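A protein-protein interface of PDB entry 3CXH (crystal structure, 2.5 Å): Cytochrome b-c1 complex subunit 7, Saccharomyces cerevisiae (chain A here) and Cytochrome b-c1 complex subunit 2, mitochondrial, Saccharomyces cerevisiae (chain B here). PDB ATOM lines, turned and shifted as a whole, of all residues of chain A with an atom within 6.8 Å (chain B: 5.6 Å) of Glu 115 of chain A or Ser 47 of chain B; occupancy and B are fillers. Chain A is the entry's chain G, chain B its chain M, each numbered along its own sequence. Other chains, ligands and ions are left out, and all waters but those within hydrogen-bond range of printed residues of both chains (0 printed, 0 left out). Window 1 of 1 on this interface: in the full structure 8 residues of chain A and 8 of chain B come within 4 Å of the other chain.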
ATOM      1  N   GLU A 110      -7.752 -25.987  24.287  1.00  0.00           N
ATOM      2  CA  GLU A 110      -7.730 -25.753  25.730  1.00  0.00           C
ATOM      3  C   GLU A 110      -7.712 -24.279  26.090  1.00  0.00           C
ATOM      4  O   GLU A 110      -8.403 -23.853  27.016  1.00  0.00           O
ATOM      5  CB  GLU A 110      -6.525 -26.437  26.377  1.00  0.00           C
ATOM      6  CG  GLU A 110      -6.657 -27.942  26.521  1.00  0.00           C
ATOM      7  CD  GLU A 110      -5.543 -28.546  27.352  1.00  0.00           C
ATOM      8  OE1 GLU A 110      -5.367 -29.784  27.323  1.00  0.00           O
ATOM      9  OE2 GLU A 110      -4.842 -27.778  28.044  1.00  0.00           O
ATOM     10  N   ALA A 111      -6.895 -23.514  25.377  1.00  0.00           N
ATOM     11  CA  ALA A 111      -6.783 -22.085  25.615  1.00  0.00           C
ATOM     12  C   ALA A 111      -8.140 -21.431  25.345  1.00  0.00           C
ATOM     13  O   ALA A 111      -8.579 -20.562  26.104  1.00  0.00           O
ATOM     14  CB  ALA A 111      -5.706 -21.489  24.726  1.00  0.00           C
ATOM     15  N   ALA A 112      -8.818 -21.902  24.297  1.00  0.00           N
ATOM     16  CA  ALA A 112     -10.135 -21.393  23.924  1.00  0.00           C
ATOM     17  C   ALA A 112     -11.171 -21.762  24.983  1.00  0.00           C
ATOM     18  O   ALA A 112     -11.980 -20.921  25.385  1.00  0.00           O
ATOM     19  CB  ALA A 112     -10.552 -21.938  22.557  1.00  0.00           C
ATOM     20  N   ALA A 113     -11.108 -23.004  25.466  1.00  0.00           N
ATOM     21  CA  ALA A 113     -12.032 -23.493  26.493  1.00  0.00           C
ATOM     22  C   ALA A 113     -11.844 -22.802  27.845  1.00  0.00           C
ATOM     23  O   ALA A 113     -12.817 -22.500  28.515  1.00  0.00           O
ATOM     24  CB  ALA A 113     -11.917 -25.005  26.647  1.00  0.00           C
ATOM     25  N   LYS A 114     -10.602 -22.547  28.243  1.00  0.00           N
ATOM     26  CA  LYS A 114     -10.351 -21.873  29.514  1.00  0.00           C
ATOM     27  C   LYS A 114     -10.870 -20.440  29.443  1.00  0.00           C
ATOM     28  O   LYS A 114     -11.451 -19.933  30.402  1.00  0.00           O
ATOM     29  CB  LYS A 114      -8.857 -21.853  29.859  1.00  0.00           C
ATOM     30  CG  LYS A 114      -8.583 -21.241  31.233  1.00  0.00           C
ATOM     31  CD  LYS A 114      -7.099 -21.198  31.597  1.00  0.00           C
ATOM     32  CE  LYS A 114      -6.314 -20.235  30.711  1.00  0.00           C
ATOM     33  NZ  LYS A 114      -4.896 -20.064  31.170  1.00  0.00           N
ATOM     34  N   GLU A 115     -10.663 -19.793  28.302  1.00  0.00           N
ATOM     35  CA  GLU A 115     -11.129 -18.429  28.131  1.00  0.00           C
ATOM     36  C   GLU A 115     -12.652 -18.390  28.255  1.00  0.00           C
ATOM     37  O   GLU A 115     -13.200 -17.503  28.922  1.00  0.00           O
ATOM     38  CB  GLU A 115     -10.693 -17.859  26.776  1.00  0.00           C
ATOM     39  CG  GLU A 115     -11.087 -16.399  26.589  1.00  0.00           C
ATOM     40  CD  GLU A 115     -10.822 -15.884  25.193  1.00  0.00           C
ATOM     41  OE1 GLU A 115     -11.151 -16.601  24.229  1.00  0.00           O
ATOM     42  OE2 GLU A 115     -10.295 -14.756  25.057  1.00  0.00           O
ATOM     43  N   LYS A 116     -13.325 -19.359  27.631  1.00  0.00           N
ATOM     44  CA  LYS A 116     -14.784 -19.430  27.690  1.00  0.00           C
ATOM     45  C   LYS A 116     -15.245 -19.632  29.126  1.00  0.00           C
ATOM     46  O   LYS A 116     -16.261 -19.088  29.538  1.00  0.00           O
ATOM     47  CB  LYS A 116     -15.326 -20.569  26.826  1.00  0.00           C
ATOM     48  CG  LYS A 116     -16.838 -20.564  26.745  1.00  0.00           C
ATOM     49  CD  LYS A 116     -17.384 -21.784  26.049  1.00  0.00           C
ATOM     50  CE  LYS A 116     -18.875 -21.626  25.767  1.00  0.00           C
ATOM     51  NZ  LYS A 116     -19.648 -21.320  26.999  1.00  0.00           N
ATOM     52  N   ASP A 117     -14.487 -20.419  29.879  1.00  0.00           N
ATOM     53  CA  ASP A 117     -14.806 -20.682  31.273  1.00  0.00           C
ATOM     54  C   ASP A 117     -14.635 -19.394  32.109  1.00  0.00           C
ATOM     55  O   ASP A 117     -15.460 -19.088  32.979  1.00  0.00           O
ATOM     56  CB  ASP A 117     -13.920 -21.825  31.778  1.00  0.00           C
ATOM     57  CG  ASP A 117     -14.109 -22.112  33.255  1.00  0.00           C
ATOM     58  OD1 ASP A 117     -15.134 -22.740  33.620  1.00  0.00           O
ATOM     59  OD2 ASP A 117     -13.222 -21.708  34.050  1.00  0.00           O
ATOM     60  N   GLU A 118     -13.586 -18.628  31.811  1.00  0.00           N
ATOM     61  CA  GLU A 118     -13.314 -17.362  32.501  1.00  0.00           C
ATOM     62  C   GLU A 118     -14.387 -16.329  32.151  1.00  0.00           C
ATOM     63  O   GLU A 118     -14.848 -15.588  33.016  1.00  0.00           O
ATOM     64  CB  GLU A 118     -11.944 -16.796  32.099  1.00  0.00           C
ATOM     65  CG  GLU A 118     -10.728 -17.535  32.642  1.00  0.00           C
ATOM     66  CD  GLU A 118      -9.446 -17.209  31.864  1.00  0.00           C
ATOM     67  OE1 GLU A 118      -9.440 -16.226  31.087  1.00  0.00           O
ATOM     68  OE2 GLU A 118      -8.444 -17.947  32.012  1.00  0.00           O
ATOM     69  N   LEU A 119     -14.769 -16.283  30.877  1.00  0.00           N
ATOM     70  CA  LEU A 119     -15.784 -15.343  30.419  1.00  0.00           C
ATOM     71  C   LEU A 119     -17.201 -15.704  30.853  1.00  0.00           C
ATOM     72  O   LEU A 119     -18.066 -14.829  30.932  1.00  0.00           O
ATOM     73  CB  LEU A 119     -15.716 -15.168  28.900  1.00  0.00           C
ATOM     74  CG  LEU A 119     -14.415 -14.531  28.393  1.00  0.00           C
ATOM     75  CD1 LEU A 119     -14.409 -14.472  26.877  1.00  0.00           C
ATOM     76  CD2 LEU A 119     -14.236 -13.135  28.993  1.00  0.00           C
ATOM     77  N   ASP A 120     -17.455 -16.989  31.106  1.00  0.00           N
ATOM     78  CA  ASP A 120     -18.778 -17.421  31.545  1.00  0.00           C
ATOM     79  C   ASP A 120     -18.964 -17.080  33.013  1.00  0.00           C
ATOM     80  O   ASP A 120     -20.076 -17.129  33.532  1.00  0.00           O
ATOM     81  CB  ASP A 120     -18.964 -18.928  31.355  1.00  0.00           C
ATOM     82  CG  ASP A 120     -19.267 -19.315  29.917  1.00  0.00           C
ATOM     83  OD1 ASP A 120     -19.598 -18.425  29.113  1.00  0.00           O
ATOM     84  OD2 ASP A 120     -19.186 -20.519  29.588  1.00  0.00           O
ATOM     85  N   ASN A 121     -17.866 -16.731  33.679  1.00  0.00           N
ATOM     86  CA  ASN A 121     -17.914 -16.389  35.095  1.00  0.00           C
ATOM     87  C   ASN A 121     -17.248 -15.061  35.435  1.00  0.00           C
ATOM     88  O   ASN A 121     -16.813 -14.868  36.565  1.00  0.00           O
ATOM     89  CB  ASN A 121     -17.280 -17.508  35.933  1.00  0.00           C
ATOM     90  CG  ASN A 121     -17.921 -18.860  35.682  1.00  0.00           C
ATOM     91  OD1 ASN A 121     -19.005 -19.152  36.189  1.00  0.00           O
ATOM     92  ND2 ASN A 121     -17.259 -19.688  34.881  1.00  0.00           N
ATOM     93  N   GLN B  41     -14.040 -12.497  13.184  1.00  0.00           N
ATOM     94  CA  GLN B  41     -13.636 -13.807  13.652  1.00  0.00           C
ATOM     95  C   GLN B  41     -12.421 -13.517  14.549  1.00  0.00           C
ATOM     96  O   GLN B  41     -12.231 -12.380  14.993  1.00  0.00           O
ATOM     97  CB  GLN B  41     -13.238 -14.703  12.481  1.00  0.00           C
ATOM     98  CG  GLN B  41     -14.413 -15.334  11.744  1.00  0.00           C
ATOM     99  CD  GLN B  41     -15.248 -16.279  12.617  1.00  0.00           C
ATOM    100  OE1 GLN B  41     -16.480 -16.263  12.561  1.00  0.00           O
ATOM    101  NE2 GLN B  41     -14.581 -17.116  13.406  1.00  0.00           N
ATOM    102  N   ASN B  42     -11.585 -14.516  14.808  1.00  0.00           N
ATOM    103  CA  ASN B  42     -10.420 -14.297  15.662  1.00  0.00           C
ATOM    104  C   ASN B  42      -9.374 -13.348  15.074  1.00  0.00           C
ATOM    105  O   ASN B  42      -9.144 -13.333  13.862  1.00  0.00           O
ATOM    106  CB  ASN B  42      -9.717 -15.626  15.961  1.00  0.00           C
ATOM    107  CG  ASN B  42     -10.467 -16.499  16.960  1.00  0.00           C
ATOM    108  OD1 ASN B  42     -11.563 -16.172  17.416  1.00  0.00           O
ATOM    109  ND2 ASN B  42      -9.866 -17.629  17.297  1.00  0.00           N
ATOM    110  N   THR B  43      -8.801 -12.505  15.930  1.00  0.00           N
ATOM    111  CA  THR B  43      -7.701 -11.625  15.526  1.00  0.00           C
ATOM    112  C   THR B  43      -6.518 -12.238  16.291  1.00  0.00           C
ATOM    113  O   THR B  43      -6.719 -12.984  17.256  1.00  0.00           O
ATOM    114  CB  THR B  43      -7.865 -10.122  15.952  1.00  0.00           C
ATOM    115  OG1 THR B  43      -7.700  -9.986  17.367  1.00  0.00           O
ATOM    116  CG2 THR B  43      -9.219  -9.558  15.523  1.00  0.00           C
ATOM    117  N   THR B  45      -4.741 -11.194  18.522  1.00  0.00           N
ATOM    118  CA  THR B  45      -4.681 -10.854  19.945  1.00  0.00           C
ATOM    119  C   THR B  45      -5.996 -10.991  20.708  1.00  0.00           C
ATOM    120  O   THR B  45      -5.994 -11.130  21.934  1.00  0.00           O
ATOM    121  CB  THR B  45      -4.133  -9.413  20.183  1.00  0.00           C
ATOM    122  OG1 THR B  45      -5.016  -8.446  19.593  1.00  0.00           O
ATOM    123  CG2 THR B  45      -2.727  -9.260  19.593  1.00  0.00           C
ATOM    124  N   ARG B  46      -7.113 -10.941  19.993  1.00  0.00           N
ATOM    125  CA  ARG B  46      -8.428 -11.040  20.621  1.00  0.00           C
ATOM    126  C   ARG B  46      -9.338 -11.986  19.836  1.00  0.00           C
ATOM    127  O   ARG B  46      -9.482 -11.860  18.613  1.00  0.00           O
ATOM    128  CB  ARG B  46      -9.043  -9.639  20.735  1.00  0.00           C
ATOM    129  CG  ARG B  46     -10.506  -9.603  21.114  1.00  0.00           C
ATOM    130  CD  ARG B  46     -10.787  -8.730  22.343  1.00  0.00           C
ATOM    131  NE  ARG B  46     -10.568  -7.279  22.213  1.00  0.00           N
ATOM    132  CZ  ARG B  46     -10.734  -6.540  21.114  1.00  0.00           C
ATOM    133  NH1 ARG B  46     -10.517  -5.237  21.179  1.00  0.00           N
ATOM    134  NH2 ARG B  46     -11.055  -7.084  19.946  1.00  0.00           N
ATOM    135  N   SER B  47      -9.938 -12.945  20.537  1.00  0.00           N
ATOM    136  CA  SER B  47     -10.821 -13.915  19.892  1.00  0.00           C
ATOM    137  C   SER B  47     -12.202 -13.331  19.623  1.00  0.00           C
ATOM    138  O   SER B  47     -12.596 -12.325  20.226  1.00  0.00           O
ATOM    139  CB  SER B  47     -10.955 -15.181  20.750  1.00  0.00           C
ATOM    140  OG  SER B  47     -11.706 -14.927  21.926  1.00  0.00           O
ATOM    141  N   ALA B  48     -12.928 -13.971  18.712  1.00  0.00           N
ATOM    142  CA  ALA B  48     -14.285 -13.559  18.366  1.00  0.00           C
ATOM    143  C   ALA B  48     -15.152 -13.586  19.623  1.00  0.00           C
ATOM    144  O   ALA B  48     -15.953 -12.682  19.859  1.00  0.00           O
ATOM    145  CB  ALA B  48     -14.862 -14.491  17.317  1.00  0.00           C
ATOM    146  N   LEU B  49     -14.960 -14.619  20.440  1.00  0.00           N
ATOM    147  CA  LEU B  49     -15.723 -14.768  21.663  1.00  0.00           C
ATOM    148  C   LEU B  49     -15.471 -13.597  22.593  1.00  0.00           C
ATOM    149  O   LEU B  49     -16.419 -12.991  23.087  1.00  0.00           O
ATOM    150  CB  LEU B  49     -15.375 -16.083  22.365  1.00  0.00           C
ATOM    151  CG  LEU B  49     -15.942 -16.277  23.784  1.00  0.00           C
ATOM    152  CD1 LEU B  49     -17.454 -16.382  23.755  1.00  0.00           C
ATOM    153  CD2 LEU B  49     -15.340 -17.519  24.408  1.00  0.00           C
ATOM    154  N   LYS B  50     -14.202 -13.262  22.811  1.00  0.00           N
ATOM    155  CA  LYS B  50     -13.871 -12.156  23.699  1.00  0.00           C
ATOM    156  C   LYS B  50     -14.431 -10.824  23.206  1.00  0.00           C
ATOM    157  O   LYS B  50     -14.908 -10.014  24.005  1.00  0.00           O
ATOM    158  CB  LYS B  50     -12.364 -12.046  23.919  1.00  0.00           C
ATOM    159  CG  LYS B  50     -12.019 -11.023  24.986  1.00  0.00           C
ATOM    160  CD  LYS B  50     -10.578 -11.099  25.404  1.00  0.00           C
ATOM    161  CE  LYS B  50     -10.298 -10.116  26.531  1.00  0.00           C
ATOM    162  NZ  LYS B  50      -8.922 -10.300  27.065  1.00  0.00           N
ATOM    163  N   LEU B  51     -14.397 -10.618  21.892  1.00  0.00           N
ATOM    164  CA  LEU B  51     -14.909  -9.392  21.300  1.00  0.00           C
ATOM    165  C   LEU B  51     -16.394  -9.204  21.619  1.00  0.00           C
ATOM    166  O   LEU B  51     -16.803  -8.144  22.107  1.00  0.00           O
ATOM    167  CB  LEU B  51     -14.693  -9.404  19.790  1.00  0.00           C
ATOM    168  CG  LEU B  51     -15.053  -8.109  19.058  1.00  0.00           C
ATOM    169  CD1 LEU B  51     -14.228  -6.965  19.611  1.00  0.00           C
ATOM    170  CD2 LEU B  51     -14.817  -8.267  17.569  1.00  0.00           C
ATOM    171  N   VAL B  52     -17.182 -10.254  21.388  1.00  0.00           N
ATOM    172  CA  VAL B  52     -18.618 -10.223  21.647  1.00  0.00           C
ATOM    173  C   VAL B  52     -18.942 -10.017  23.132  1.00  0.00           C
ATOM    174  O   VAL B  52     -19.695  -9.109  23.489  1.00  0.00           O
ATOM    175  CB  VAL B  52     -19.313 -11.515  21.129  1.00  0.00           C
ATOM    176  CG1 VAL B  52     -20.757 -11.581  21.602  1.00  0.00           C
ATOM    177  CG2 VAL B  52     -19.269 -11.564  19.625  1.00  0.00           C
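The side-chain hydroxyl (OG) of Ser 47 of chain B sits at hydrogen-bond distance from the side-chain carboxylate (OE1) of Glu 115 of chain A, 2.9 Å away.
The side-chain hydroxyl (OG) of Ser 47 of chain B sits at hydrogen-bond distance from the backbone NH (N) of Lys 50 of chain B.
The side-chain amino group (NZ) of Lys 116 of chain A is in salt-bridge range of the side-chain carboxylate (OD2) of Asp 120 of chain A (2.7 Å).
Glu 115 of chain A touches Lys 50 of chain B.
CA of Lys 116 of chain A touches CD2 of Leu 49 of chain B, 3.8 Å away.
Leu 119 of chain A touches Leu 49 of chain B.
CA of Lys 50 of chain B touches CD1 of Leu 119 of chain A, at 3.97 Å.
Ala 113 of chain A touches none of the printed residues of chain B.
Glu 115 of chain A touches just these residues of chain B: Ser 47 (2.9 Å) and Lys 50 (3.6 Å).
Printed residues of chain B within 4 Å of Lys 116 of chain A: Leu 49.
Of the printed residues of chain B, Leu 119 of chain A touches Leu 49 and Lys 50.
Asn 121 of chain A touches none of the printed residues of chain B.
Of chain A, only Glu 115 comes within 4 Å of Ser 47 of chain B.
Of the printed residues of chain A, Lys 50 of chain B touches Glu 115 (3.6 Å) and Leu 119 (3.97 Å).
The nearest residue of chain B that does not touch Glu 115 of chain A is Leu 49 of chain B (4.3 Å).
The nearest printed residue of chain A that does not touch Lys 50 of chain B is Glu 118 of chain A (7.2 Å).
Printed residues of chain B that touch a printed residue of chain A: Ser 47, Leu 49 and Lys 50.
Hydrophobic or aromatic side chains of chain B that line the printed part of chain A: Leu 49.
Among the printed residues, no Asp or Glu carboxylate lies within 4 Å of a Lys or Arg side-chain nitrogen of the other chain.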
